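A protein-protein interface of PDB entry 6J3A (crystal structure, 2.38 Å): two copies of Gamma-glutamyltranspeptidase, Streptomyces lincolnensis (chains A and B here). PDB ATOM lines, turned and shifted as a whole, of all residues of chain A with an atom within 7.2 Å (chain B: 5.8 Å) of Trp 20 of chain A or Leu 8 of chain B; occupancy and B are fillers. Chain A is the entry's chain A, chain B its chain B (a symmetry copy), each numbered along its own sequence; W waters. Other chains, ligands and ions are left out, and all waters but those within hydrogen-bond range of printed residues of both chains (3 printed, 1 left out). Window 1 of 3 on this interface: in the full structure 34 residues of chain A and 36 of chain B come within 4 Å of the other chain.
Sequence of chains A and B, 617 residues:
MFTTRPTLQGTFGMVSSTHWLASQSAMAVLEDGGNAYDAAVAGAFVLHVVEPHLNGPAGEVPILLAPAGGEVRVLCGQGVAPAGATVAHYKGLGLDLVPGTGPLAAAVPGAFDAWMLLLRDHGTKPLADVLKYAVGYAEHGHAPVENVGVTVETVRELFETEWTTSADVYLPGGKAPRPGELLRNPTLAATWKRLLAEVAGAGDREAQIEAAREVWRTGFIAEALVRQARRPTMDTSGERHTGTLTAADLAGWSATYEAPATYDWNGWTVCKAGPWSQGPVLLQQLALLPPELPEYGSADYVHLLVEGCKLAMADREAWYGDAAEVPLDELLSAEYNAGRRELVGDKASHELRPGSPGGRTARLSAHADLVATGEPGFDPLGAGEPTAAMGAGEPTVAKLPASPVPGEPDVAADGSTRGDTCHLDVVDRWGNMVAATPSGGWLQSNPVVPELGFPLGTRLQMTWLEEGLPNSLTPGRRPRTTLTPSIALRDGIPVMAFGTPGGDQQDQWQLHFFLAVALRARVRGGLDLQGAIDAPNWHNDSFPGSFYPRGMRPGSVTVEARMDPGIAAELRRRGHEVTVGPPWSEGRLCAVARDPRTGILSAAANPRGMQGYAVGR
NE1 of Trp 20 of chain A is in hydrogen-bond range of O of Gln 9 of chain B (2.9 Å).
The guanidinium group (NH2) of Arg 524 of chain B lies within hydrogen-bond range of the backbone carbonyl oxygen (O) of Gly 609 of chain A (3.1 Å).
O of Met 610 of chain A lies within hydrogen-bond range of NH1 of Arg 524 of chain B (2.8 Å).
The backbone carbonyl oxygen of Ala 614 of chain B is in hydrogen-bond range of the side-chain hydroxyl of Tyr 613 of chain A (2.6 Å).
A ring nitrogen (ND1) of His 19 of chain A lies close to the backbone NH of Leu 21 of chain A.
The backbone carbonyl oxygen (O) of Leu 21 of chain A sits at hydrogen-bond distance from the side-chain hydroxyl (OG) of Ser 25 of chain A (2.6 Å).
Among the printed residues, merely in contact across the chains: Trp 20 of chain A with Leu 8 of chain B (3.98 Å), Trp 20 of chain A with Arg 524 of chain B (3.7 Å), Trp 20 of chain A with Gly 616 of chain B (3.7 Å), Leu 21 of chain A with Gln 9 of chain B (3.6 Å), Leu 21 of chain A with Arg 617 of chain B (3.7 Å), Gln 24 of chain A with Gly 616 of chain B (3.9 Å), Gln 24 of chain A with Arg 617 of chain B (3.7 Å), Ser 25 of chain A with Arg 617 of chain B (3.7 Å), Ala 143 of chain A with Gln 9 of chain B (3.9 Å), Val 145 of chain A with Arg 524 of chain B (3.8 Å), Met 610 of chain A with Pro 6 of chain B (3.3 Å) and Tyr 613 of chain A with Pro 6 of chain B (3.8 Å).
Trp 20 of chain A touches four residues of chain B.
Pro 144 of chain A touches none of the printed residues of chain B.
Of the printed residues of chain B, Val 145 of chain A touches Arg 524 (3.8 Å).
Printed residues of chain B within 4 Å of Met 610 of chain A: Pro 6 and Arg 524.
Printed residues of chain A within 4 Å of Pro 6 of chain B: Met 610 (3.3 Å) and Tyr 613 (3.8 Å).
Leu 8 of chain B touches one residue of chain A.
Ser 602 of chain B touches none of the printed residues of chain A.
The nearest residue of chain A that does not touch Leu 8 of chain B is Tyr 613 of chain A (4.1 Å).
Hydrophobic or aromatic side chains of chain A that line the printed part of chain B: Trp 20, Leu 21, Ala 143, Val 145, Met 610 and Tyr 613.
Of the 15 printed residues of chain B, 7 touch a printed residue of chain A.
Printed residues of chain B that touch a printed residue of chain A: Pro 6, Leu 8, Gln 9, Arg 524, Ala 614, Gly 616 and Arg 617.
Among the printed residues, no Asp or Glu carboxylate lies within 4 Å of a Lys or Arg side-chain nitrogen of the other chain.
Positions printed for both chains: 614 and 615.
Of the 16 pairs that touch across the chains among the printed residues, none has its exchanged pair printed and touching as well.
Water W2 bridges the side-chain amide oxygen of Gln 24 of chain A (2.7 Å) and the backbone NH of Gly 616 of chain B (2.9 Å).
Water W1 bridges the backbone NH of Ala 143 of chain A and the backbone carbonyl oxygen of Gln 9 of chain B.
Water W3 lies within hydrogen-bond range of the side-chain hydroxyl of Tyr 613 of chain A and the backbone NH of Ala 614 of chain B.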
ATOM      1  N   SER A  17       7.573 -22.978 -27.771  1.00  0.00           N
ATOM      2  CA  SER A  17       7.838 -24.377 -28.110  1.00  0.00           C
ATOM      3  C   SER A  17       6.576 -25.202 -28.103  1.00  0.00           C
ATOM      4  O   SER A  17       5.496 -24.740 -27.722  1.00  0.00           O
ATOM      5  CB  SER A  17       8.789 -25.020 -27.094  1.00  0.00           C
ATOM      6  OG  SER A  17      10.110 -24.616 -27.323  1.00  0.00           O
ATOM      7  N   THR A  18       6.759 -26.450 -28.520  1.00  0.00           N
ATOM      8  CA  THR A  18       5.778 -27.517 -28.351  1.00  0.00           C
ATOM      9  C   THR A  18       5.899 -28.225 -26.995  1.00  0.00           C
ATOM     10  O   THR A  18       5.199 -29.212 -26.778  1.00  0.00           O
ATOM     11  CB  THR A  18       5.902 -28.577 -29.480  1.00  0.00           C
ATOM     12  OG1 THR A  18       7.262 -29.020 -29.595  1.00  0.00           O
ATOM     13  CG2 THR A  18       5.448 -28.006 -30.802  1.00  0.00           C
ATOM     14  N   HIS A  19       6.767 -27.723 -26.102  1.00  0.00           N
ATOM     15  CA  HIS A  19       6.952 -28.251 -24.744  1.00  0.00           C
ATOM     16  C   HIS A  19       7.531 -27.216 -23.774  1.00  0.00           C
ATOM     17  O   HIS A  19       8.595 -26.634 -24.019  1.00  0.00           O
ATOM     18  CB  HIS A  19       7.869 -29.461 -24.761  1.00  0.00           C
ATOM     19  CG  HIS A  19       7.644 -30.406 -23.625  1.00  0.00           C
ATOM     20  ND1 HIS A  19       7.919 -30.081 -22.315  1.00  0.00           N
ATOM     21  CD2 HIS A  19       7.190 -31.681 -23.610  1.00  0.00           C
ATOM     22  CE1 HIS A  19       7.637 -31.112 -21.540  1.00  0.00           C
ATOM     23  NE2 HIS A  19       7.190 -32.094 -22.300  1.00  0.00           N
ATOM     24  N   TRP A  20       6.844 -27.037 -22.648  1.00  0.00           N
ATOM     25  CA  TRP A  20       7.142 -25.968 -21.681  1.00  0.00           C
ATOM     26  C   TRP A  20       8.573 -26.034 -21.119  1.00  0.00           C
ATOM     27  O   TRP A  20       9.205 -25.002 -20.896  1.00  0.00           O
ATOM     28  CB  TRP A  20       6.105 -25.963 -20.530  1.00  0.00           C
ATOM     29  CG  TRP A  20       6.208 -27.140 -19.609  1.00  0.00           C
ATOM     30  CD1 TRP A  20       7.018 -27.259 -18.513  1.00  0.00           C
ATOM     31  CD2 TRP A  20       5.487 -28.373 -19.711  1.00  0.00           C
ATOM     32  NE1 TRP A  20       6.855 -28.493 -17.934  1.00  0.00           N
ATOM     33  CE2 TRP A  20       5.924 -29.201 -18.649  1.00  0.00           C
ATOM     34  CE3 TRP A  20       4.527 -28.869 -20.606  1.00  0.00           C
ATOM     35  CZ2 TRP A  20       5.421 -30.496 -18.449  1.00  0.00           C
ATOM     36  CZ3 TRP A  20       4.028 -30.155 -20.406  1.00  0.00           C
ATOM     37  CH2 TRP A  20       4.475 -30.952 -19.335  1.00  0.00           C
ATOM     38  N   LEU A  21       9.055 -27.253 -20.891  1.00  0.00           N
ATOM     39  CA  LEU A  21      10.398 -27.490 -20.383  1.00  0.00           C
ATOM     40  C   LEU A  21      11.447 -26.930 -21.337  1.00  0.00           C
ATOM     41  O   LEU A  21      12.443 -26.337 -20.908  1.00  0.00           O
ATOM     42  CB  LEU A  21      10.631 -28.993 -20.167  1.00  0.00           C
ATOM     43  CG  LEU A  21       9.858 -29.723 -19.052  1.00  0.00           C
ATOM     44  CD1 LEU A  21      10.140 -31.213 -19.122  1.00  0.00           C
ATOM     45  CD2 LEU A  21      10.199 -29.222 -17.661  1.00  0.00           C
ATOM     46  N   ALA A  22      11.201 -27.101 -22.633  1.00  0.00           N
ATOM     47  CA  ALA A  22      12.114 -26.596 -23.654  1.00  0.00           C
ATOM     48  C   ALA A  22      12.017 -25.076 -23.781  1.00  0.00           C
ATOM     49  O   ALA A  22      13.030 -24.399 -23.979  1.00  0.00           O
ATOM     50  CB  ALA A  22      11.832 -27.266 -24.985  1.00  0.00           C
ATOM     51  N   SER A  23      10.803 -24.544 -23.661  1.00  0.00           N
ATOM     52  CA  SER A  23      10.596 -23.098 -23.705  1.00  0.00           C
ATOM     53  C   SER A  23      11.381 -22.414 -22.613  1.00  0.00           C
ATOM     54  O   SER A  23      12.166 -21.500 -22.880  1.00  0.00           O
ATOM     55  CB  SER A  23       9.129 -22.759 -23.528  1.00  0.00           C
ATOM     56  OG  SER A  23       8.394 -23.101 -24.674  1.00  0.00           O
ATOM     57  N   GLN A  24      11.166 -22.882 -21.384  1.00  0.00           N
ATOM     58  CA  GLN A  24      11.750 -22.255 -20.205  1.00  0.00           C
ATOM     59  C   GLN A  24      13.264 -22.440 -20.150  1.00  0.00           C
ATOM     60  O   GLN A  24      13.971 -21.586 -19.610  1.00  0.00           O
ATOM     61  CB  GLN A  24      11.083 -22.792 -18.928  1.00  0.00           C
ATOM     62  CG  GLN A  24      11.513 -22.140 -17.609  1.00  0.00           C
ATOM     63  CD  GLN A  24      11.607 -20.618 -17.670  1.00  0.00           C
ATOM     64  OE1 GLN A  24      10.616 -19.943 -17.941  1.00  0.00           O
ATOM     65  NE2 GLN A  24      12.813 -20.072 -17.421  1.00  0.00           N
ATOM     66  N   SER A  25      13.752 -23.544 -20.716  1.00  0.00           N
ATOM     67  CA  SER A  25      15.185 -23.830 -20.744  1.00  0.00           C
ATOM     68  C   SER A  25      15.868 -22.865 -21.709  1.00  0.00           C
ATOM     69  O   SER A  25      16.920 -22.301 -21.397  1.00  0.00           O
ATOM     70  CB  SER A  25      15.461 -25.284 -21.154  1.00  0.00           C
ATOM     71  OG  SER A  25      14.982 -26.206 -20.189  1.00  0.00           O
ATOM     72  N   ALA A  26      15.251 -22.673 -22.874  1.00  0.00           N
ATOM     73  CA  ALA A  26      15.711 -21.681 -23.850  1.00  0.00           C
ATOM     74  C   ALA A  26      15.658 -20.260 -23.276  1.00  0.00           C
ATOM     75  O   ALA A  26      16.558 -19.453 -23.490  1.00  0.00           O
ATOM     76  CB  ALA A  26      14.868 -21.769 -25.108  1.00  0.00           C
ATOM     77  N   VAL A  46      16.886 -30.062 -25.220  1.00  0.00           N
ATOM     78  CA  VAL A  46      15.847 -30.377 -24.247  1.00  0.00           C
ATOM     79  C   VAL A  46      14.698 -31.126 -24.943  1.00  0.00           C
ATOM     80  O   VAL A  46      14.223 -32.137 -24.429  1.00  0.00           O
ATOM     81  CB  VAL A  46      15.371 -29.113 -23.494  1.00  0.00           C
ATOM     82  CG1 VAL A  46      14.106 -29.381 -22.687  1.00  0.00           C
ATOM     83  CG2 VAL A  46      16.482 -28.616 -22.574  1.00  0.00           C
ATOM     84  N   LEU A  47      14.289 -30.657 -26.118  1.00  0.00           N
ATOM     85  CA  LEU A  47      13.234 -31.332 -26.885  1.00  0.00           C
ATOM     86  C   LEU A  47      13.519 -32.800 -27.189  1.00  0.00           C
ATOM     87  O   LEU A  47      12.593 -33.622 -27.184  1.00  0.00           O
ATOM     88  CB  LEU A  47      12.955 -30.599 -28.196  1.00  0.00           C
ATOM     89  CG  LEU A  47      12.169 -29.296 -28.095  1.00  0.00           C
ATOM     90  CD1 LEU A  47      12.217 -28.570 -29.427  1.00  0.00           C
ATOM     91  CD2 LEU A  47      10.727 -29.556 -27.694  1.00  0.00           C
ATOM     92  N   VAL A  50      12.562 -34.459 -23.879  1.00  0.00           N
ATOM     93  CA  VAL A  50      11.167 -34.354 -23.419  1.00  0.00           C
ATOM     94  C   VAL A  50      10.108 -34.685 -24.462  1.00  0.00           C
ATOM     95  O   VAL A  50       8.938 -34.807 -24.111  1.00  0.00           O
ATOM     96  CB  VAL A  50      10.871 -32.982 -22.776  1.00  0.00           C
ATOM     97  CG1 VAL A  50      11.897 -32.695 -21.682  1.00  0.00           C
ATOM     98  CG2 VAL A  50      10.823 -31.857 -23.811  1.00  0.00           C
ATOM     99  N   GLU A  51      10.516 -34.820 -25.725  1.00  0.00           N
ATOM    100  CA  GLU A  51       9.649 -35.330 -26.790  1.00  0.00           C
ATOM    101  C   GLU A  51      10.371 -36.385 -27.650  1.00  0.00           C
ATOM    102  O   GLU A  51      10.424 -36.264 -28.878  1.00  0.00           O
ATOM    103  CB  GLU A  51       9.153 -34.182 -27.669  1.00  0.00           C
ATOM    104  CG  GLU A  51       8.432 -33.082 -26.909  1.00  0.00           C
ATOM    105  CD  GLU A  51       7.598 -32.184 -27.808  1.00  0.00           C
ATOM    106  OE1 GLU A  51       6.703 -32.702 -28.509  1.00  0.00           O
ATOM    107  OE2 GLU A  51       7.821 -30.957 -27.807  1.00  0.00           O
ATOM    108  N   HIS A 142      12.480 -36.175 -15.910  1.00  0.00           N
ATOM    109  CA  HIS A 142      11.346 -35.265 -16.040  1.00  0.00           C
ATOM    110  C   HIS A 142      10.003 -36.001 -16.065  1.00  0.00           C
ATOM    111  O   HIS A 142       9.917 -37.147 -16.487  1.00  0.00           O
ATOM    112  CB  HIS A 142      11.499 -34.427 -17.306  1.00  0.00           C
ATOM    113  CG  HIS A 142      10.967 -35.095 -18.530  1.00  0.00           C
ATOM    114  ND1 HIS A 142      11.694 -36.022 -19.242  1.00  0.00           N
ATOM    115  CD2 HIS A 142       9.768 -34.987 -19.154  1.00  0.00           C
ATOM    116  CE1 HIS A 142      10.970 -36.451 -20.262  1.00  0.00           C
ATOM    117  NE2 HIS A 142       9.795 -35.842 -20.228  1.00  0.00           N
ATOM    118  N   ALA A 143       8.955 -35.314 -15.638  1.00  0.00           N
ATOM    119  CA  ALA A 143       7.612 -35.882 -15.619  1.00  0.00           C
ATOM    120  C   ALA A 143       7.019 -35.820 -17.024  1.00  0.00           C
ATOM    121  O   ALA A 143       6.635 -34.752 -17.488  1.00  0.00           O
ATOM    122  CB  ALA A 143       6.737 -35.139 -14.618  1.00  0.00           C
ATOM    123  N   PRO A 144       6.948 -36.966 -17.711  1.00  0.00           N
ATOM    124  CA  PRO A 144       6.609 -36.908 -19.126  1.00  0.00           C
ATOM    125  C   PRO A 144       5.132 -36.711 -19.377  1.00  0.00           C
ATOM    126  O   PRO A 144       4.309 -36.986 -18.515  1.00  0.00           O
ATOM    127  CB  PRO A 144       7.017 -38.287 -19.628  1.00  0.00           C
ATOM    128  CG  PRO A 144       6.728 -39.168 -18.462  1.00  0.00           C
ATOM    129  CD  PRO A 144       7.063 -38.357 -17.241  1.00  0.00           C
ATOM    130  N   VAL A 145       4.830 -36.252 -20.580  1.00  0.00           N
ATOM    131  CA  VAL A 145       3.469 -36.218 -21.107  1.00  0.00           C
ATOM    132  C   VAL A 145       3.004 -37.659 -21.364  1.00  0.00           C
ATOM    133  O   VAL A 145       3.824 -38.545 -21.625  1.00  0.00           O
ATOM    134  CB  VAL A 145       3.440 -35.388 -22.412  1.00  0.00           C
ATOM    135  CG1 VAL A 145       2.097 -35.467 -23.142  1.00  0.00           C
ATOM    136  CG2 VAL A 145       3.764 -33.937 -22.102  1.00  0.00           C
ATOM    137  N   GLY A 609      -3.468 -30.388 -26.403  1.00  0.00           N
ATOM    138  CA  GLY A 609      -2.562 -31.406 -25.857  1.00  0.00           C
ATOM    139  C   GLY A 609      -1.829 -30.967 -24.596  1.00  0.00           C
ATOM    140  O   GLY A 609      -0.943 -31.664 -24.133  1.00  0.00           O
ATOM    141  N   MET A 610      -2.229 -29.826 -24.032  1.00  0.00           N
ATOM    142  CA  MET A 610      -1.606 -29.207 -22.844  1.00  0.00           C
ATOM    143  C   MET A 610      -0.104 -29.456 -22.716  1.00  0.00           C
ATOM    144  O   MET A 610       0.366 -30.101 -21.777  1.00  0.00           O
ATOM    145  CB  MET A 610      -2.334 -29.578 -21.538  1.00  0.00           C
ATOM    146  CG  MET A 610      -3.554 -30.448 -21.673  1.00  0.00           C
ATOM    147  SD  MET A 610      -4.926 -29.772 -22.616  1.00  0.00           S
ATOM    148  CE  MET A 610      -5.640 -31.369 -23.032  1.00  0.00           C
ATOM    149  N   GLN A 611       0.637 -28.911 -23.667  1.00  0.00           N
ATOM    150  CA  GLN A 611       2.065 -29.184 -23.775  1.00  0.00           C
ATOM    151  C   GLN A 611       2.832 -27.996 -24.346  1.00  0.00           C
ATOM    152  O   GLN A 611       3.823 -27.551 -23.754  1.00  0.00           O
ATOM    153  CB  GLN A 611       2.269 -30.430 -24.635  1.00  0.00           C
ATOM    154  CG  GLN A 611       3.661 -31.028 -24.585  1.00  0.00           C
ATOM    155  CD  GLN A 611       3.820 -32.164 -25.580  1.00  0.00           C
ATOM    156  OE1 GLN A 611       4.819 -32.238 -26.293  1.00  0.00           O
ATOM    157  NE2 GLN A 611       2.812 -33.037 -25.659  1.00  0.00           N
ATOM    158  N   GLY A 612       2.382 -27.511 -25.501  1.00  0.00           N
ATOM    159  CA  GLY A 612       2.917 -26.306 -26.115  1.00  0.00           C
ATOM    160  C   GLY A 612       2.787 -25.128 -25.164  1.00  0.00           C
ATOM    161  O   GLY A 612       1.796 -25.011 -24.420  1.00  0.00           O
ATOM    162  N   TYR A 613       3.794 -24.259 -25.160  1.00  0.00           N
ATOM    163  CA  TYR A 613       3.834 -23.179 -24.181  1.00  0.00           C
ATOM    164  C   TYR A 613       4.794 -22.076 -24.607  1.00  0.00           C
ATOM    165  O   TYR A 613       5.899 -22.362 -25.096  1.00  0.00           O
ATOM    166  CB  TYR A 613       4.215 -23.728 -22.789  1.00  0.00           C
ATOM    167  CG  TYR A 613       3.566 -22.985 -21.629  1.00  0.00           C
ATOM    168  CD1 TYR A 613       2.164 -22.961 -21.471  1.00  0.00           C
ATOM    169  CD2 TYR A 613       4.350 -22.324 -20.675  1.00  0.00           C
ATOM    170  CE1 TYR A 613       1.566 -22.284 -20.398  1.00  0.00           C
ATOM    171  CE2 TYR A 613       3.770 -21.648 -19.600  1.00  0.00           C
ATOM    172  CZ  TYR A 613       2.383 -21.623 -19.455  1.00  0.00           C
ATOM    173  OH  TYR A 613       1.830 -20.941 -18.385  1.00  0.00           O
ATOM    174  N   ALA A 614       4.343 -20.831 -24.428  1.00  0.00           N
ATOM    175  CA  ALA A 614       5.171 -19.647 -24.629  1.00  0.00           C
ATOM    176  C   ALA A 614       5.651 -19.070 -23.291  1.00  0.00           C
ATOM    177  O   ALA A 614       4.928 -19.124 -22.287  1.00  0.00           O
ATOM    178  CB  ALA A 614       4.405 -18.590 -25.412  1.00  0.00           C
ATOM    179  N   VAL A 615       6.872 -18.539 -23.277  1.00  0.00           N
ATOM    180  CA  VAL A 615       7.380 -17.792 -22.115  1.00  0.00           C
ATOM    181  C   VAL A 615       8.168 -16.571 -22.566  1.00  0.00           C
ATOM    182  O   VAL A 615       8.835 -16.602 -23.602  1.00  0.00           O
ATOM    183  CB  VAL A 615       8.253 -18.652 -21.150  1.00  0.00           C
ATOM    184  CG1 VAL A 615       7.517 -19.918 -20.749  1.00  0.00           C
ATOM    185  CG2 VAL A 615       9.613 -19.015 -21.741  1.00  0.00           C
ATOM    186  N   PRO B   6      -1.300 -26.199 -19.571  1.00  0.00           N
ATOM    187  CA  PRO B   6      -1.009 -27.426 -18.850  1.00  0.00           C
ATOM    188  C   PRO B   6      -0.940 -27.135 -17.376  1.00  0.00           C
ATOM    189  O   PRO B   6      -0.831 -25.972 -16.989  1.00  0.00           O
ATOM    190  CB  PRO B   6       0.370 -27.850 -19.367  1.00  0.00           C
ATOM    191  CG  PRO B   6       0.887 -26.743 -20.204  1.00  0.00           C
ATOM    192  CD  PRO B   6      -0.191 -25.746 -20.429  1.00  0.00           C
ATOM    193  N   THR B   7      -1.032 -28.175 -16.558  1.00  0.00           N
ATOM    194  CA  THR B   7      -0.481 -28.089 -15.220  1.00  0.00           C
ATOM    195  C   THR B   7       1.010 -28.391 -15.394  1.00  0.00           C
ATOM    196  O   THR B   7       1.407 -29.542 -15.514  1.00  0.00           O
ATOM    197  CB  THR B   7      -1.175 -29.043 -14.246  1.00  0.00           C
ATOM    198  OG1 THR B   7      -2.575 -28.748 -14.220  1.00  0.00           O
ATOM    199  CG2 THR B   7      -0.625 -28.880 -12.849  1.00  0.00           C
ATOM    200  N   LEU B   8       1.830 -27.346 -15.447  1.00  0.00           N
ATOM    201  CA  LEU B   8       3.286 -27.524 -15.671  1.00  0.00           C
ATOM    202  C   LEU B   8       3.854 -28.463 -14.642  1.00  0.00           C
ATOM    203  O   LEU B   8       3.446 -28.421 -13.502  1.00  0.00           O
ATOM    204  CB  LEU B   8       4.073 -26.216 -15.565  1.00  0.00           C
ATOM    205  CG  LEU B   8       3.548 -24.997 -16.316  1.00  0.00           C
ATOM    206  CD1 LEU B   8       4.568 -23.870 -16.269  1.00  0.00           C
ATOM    207  CD2 LEU B   8       3.179 -25.366 -17.741  1.00  0.00           C
ATOM    208  N   GLN B   9       4.785 -29.309 -15.061  1.00  0.00           N
ATOM    209  CA  GLN B   9       5.475 -30.253 -14.182  1.00  0.00           C
ATOM    210  C   GLN B   9       6.990 -30.140 -14.396  1.00  0.00           C
ATOM    211  O   GLN B   9       7.458 -30.002 -15.522  1.00  0.00           O
ATOM    212  CB  GLN B   9       4.983 -31.667 -14.472  1.00  0.00           C
ATOM    213  CG  GLN B   9       3.613 -31.981 -13.876  1.00  0.00           C
ATOM    214  CD  GLN B   9       3.070 -33.330 -14.333  1.00  0.00           C
ATOM    215  OE1 GLN B   9       3.073 -33.648 -15.528  1.00  0.00           O
ATOM    216  NE2 GLN B   9       2.590 -34.120 -13.388  1.00  0.00           N
ATOM    217  N   GLY B  10       7.767 -30.195 -13.326  1.00  0.00           N
ATOM    218  CA  GLY B  10       9.201 -29.937 -13.454  1.00  0.00           C
ATOM    219  C   GLY B  10       9.968 -30.248 -12.202  1.00  0.00           C
ATOM    220  O   GLY B  10       9.414 -30.812 -11.267  1.00  0.00           O
ATOM    221  N   MET B  14       8.923 -23.409  -9.980  1.00  0.00           N
ATOM    222  CA  MET B  14       7.610 -23.042 -10.495  1.00  0.00           C
ATOM    223  C   MET B  14       7.224 -21.696  -9.907  1.00  0.00           C
ATOM    224  O   MET B  14       7.500 -21.412  -8.736  1.00  0.00           O
ATOM    225  CB  MET B  14       6.550 -24.091 -10.156  1.00  0.00           C
ATOM    226  CG  MET B  14       6.711 -25.427 -10.865  1.00  0.00           C
ATOM    227  SD  MET B  14       6.335 -25.358 -12.624  1.00  0.00           S
ATOM    228  CE  MET B  14       7.247 -26.791 -13.205  1.00  0.00           C
ATOM    229  N   ARG B 524      -2.081 -36.602 -15.154  1.00  0.00           N
ATOM    230  CA  ARG B 524      -0.646 -36.851 -15.342  1.00  0.00           C
ATOM    231  C   ARG B 524       0.011 -37.243 -14.030  1.00  0.00           C
ATOM    232  O   ARG B 524       1.131 -36.822 -13.735  1.00  0.00           O
ATOM    233  CB  ARG B 524       0.069 -35.625 -15.962  1.00  0.00           C
ATOM    234  CG  ARG B 524      -0.312 -35.355 -17.410  1.00  0.00           C
ATOM    235  CD  ARG B 524       0.521 -34.264 -18.071  1.00  0.00           C
ATOM    236  NE  ARG B 524       0.086 -34.076 -19.457  1.00  0.00           N
ATOM    237  CZ  ARG B 524       0.270 -32.987 -20.202  1.00  0.00           C
ATOM    238  NH1 ARG B 524       0.901 -31.911 -19.720  1.00  0.00           N
ATOM    239  NH2 ARG B 524      -0.198 -32.974 -21.453  1.00  0.00           N
ATOM    240  N   LEU B 601       7.667 -30.619  -8.954  1.00  0.00           N
ATOM    241  CA  LEU B 601       7.032 -29.324  -8.761  1.00  0.00           C
ATOM    242  C   LEU B 601       6.032 -29.123  -9.873  1.00  0.00           C
ATOM    243  O   LEU B 601       6.278 -29.531 -11.004  1.00  0.00           O
ATOM    244  CB  LEU B 601       8.075 -28.215  -8.834  1.00  0.00           C
ATOM    245  CG  LEU B 601       9.373 -28.450  -8.063  1.00  0.00           C
ATOM    246  CD1 LEU B 601      10.351 -27.295  -8.164  1.00  0.00           C
ATOM    247  CD2 LEU B 601       9.040 -28.711  -6.614  1.00  0.00           C
ATOM    248  N   SER B 602       4.911 -28.490  -9.563  1.00  0.00           N
ATOM    249  CA  SER B 602       3.935 -28.162 -10.587  1.00  0.00           C
ATOM    250  C   SER B 602       3.382 -26.745 -10.426  1.00  0.00           C
ATOM    251  O   SER B 602       3.621 -26.082  -9.423  1.00  0.00           O
ATOM    252  CB  SER B 602       2.814 -29.201 -10.602  1.00  0.00           C
ATOM    253  OG  SER B 602       2.097 -29.164  -9.395  1.00  0.00           O
ATOM    254  N   ALA B 603       2.679 -26.269 -11.442  1.00  0.00           N
ATOM    255  CA  ALA B 603       2.068 -24.946 -11.394  1.00  0.00           C
ATOM    256  C   ALA B 603       0.873 -24.863 -12.321  1.00  0.00           C
ATOM    257  O   ALA B 603       0.774 -25.613 -13.297  1.00  0.00           O
ATOM    258  CB  ALA B 603       3.079 -23.881 -11.758  1.00  0.00           C
ATOM    259  N   ALA B 604      -0.030 -23.950 -11.990  1.00  0.00           N
ATOM    260  CA  ALA B 604      -1.152 -23.607 -12.846  1.00  0.00           C
ATOM    261  C   ALA B 604      -1.494 -22.130 -12.641  1.00  0.00           C
ATOM    262  O   ALA B 604      -1.053 -21.509 -11.672  1.00  0.00           O
ATOM    263  CB  ALA B 604      -2.350 -24.506 -12.574  1.00  0.00           C
ATOM    264  N   ALA B 614       1.533 -19.034 -15.249  1.00  0.00           N
ATOM    265  CA  ALA B 614       2.507 -19.875 -14.581  1.00  0.00           C
ATOM    266  C   ALA B 614       3.755 -20.048 -15.455  1.00  0.00           C
ATOM    267  O   ALA B 614       3.667 -20.060 -16.691  1.00  0.00           O
ATOM    268  CB  ALA B 614       1.889 -21.229 -14.273  1.00  0.00           C
ATOM    269  N   VAL B 615       4.918 -20.156 -14.814  1.00  0.00           N
ATOM    270  CA  VAL B 615       6.157 -20.543 -15.508  1.00  0.00           C
ATOM    271  C   VAL B 615       7.016 -21.451 -14.626  1.00  0.00           C
ATOM    272  O   VAL B 615       7.066 -21.277 -13.408  1.00  0.00           O
ATOM    273  CB  VAL B 615       7.026 -19.337 -15.975  1.00  0.00           C
ATOM    274  CG1 VAL B 615       6.243 -18.419 -16.907  1.00  0.00           C
ATOM    275  CG2 VAL B 615       7.611 -18.560 -14.799  1.00  0.00           C
ATOM    276  N   GLY B 616       7.700 -22.402 -15.254  1.00  0.00           N
ATOM    277  CA  GLY B 616       8.632 -23.270 -14.548  1.00  0.00           C
ATOM    278  C   GLY B 616       9.147 -24.429 -15.369  1.00  0.00           C
ATOM    279  O   GLY B 616       8.718 -24.639 -16.510  1.00  0.00           O
ATOM    280  N   ARG B 617      10.081 -25.174 -14.772  1.00  0.00           N
ATOM    281  CA  ARG B 617      10.689 -26.343 -15.407  1.00  0.00           C
ATOM    282  C   ARG B 617      11.323 -27.264 -14.383  1.00  0.00           C
ATOM    283  O   ARG B 617      11.325 -26.951 -13.196  1.00  0.00           O
ATOM    284  CB  ARG B 617      11.748 -25.900 -16.403  1.00  0.00           C
ATOM    285  CG  ARG B 617      12.956 -25.229 -15.770  1.00  0.00           C
ATOM    286  CD  ARG B 617      13.960 -24.871 -16.845  1.00  0.00           C
ATOM    287  NE  ARG B 617      15.161 -24.250 -16.293  1.00  0.00           N
ATOM    288  CZ  ARG B 617      16.211 -24.908 -15.795  1.00  0.00           C
ATOM    289  NH1 ARG B 617      16.240 -26.247 -15.759  1.00  0.00           N
ATOM    290  NH2 ARG B 617      17.248 -24.219 -15.320  1.00  0.00           N
HETATM  291  O   HOH W   1       8.311 -32.822 -16.403  1.00  0.00           O
HETATM  292  O   HOH W   2       8.419 -21.460 -17.946  1.00  0.00           O
HETATM  293  O   HOH W   3      -0.480 -20.742 -17.001  1.00  0.00           O
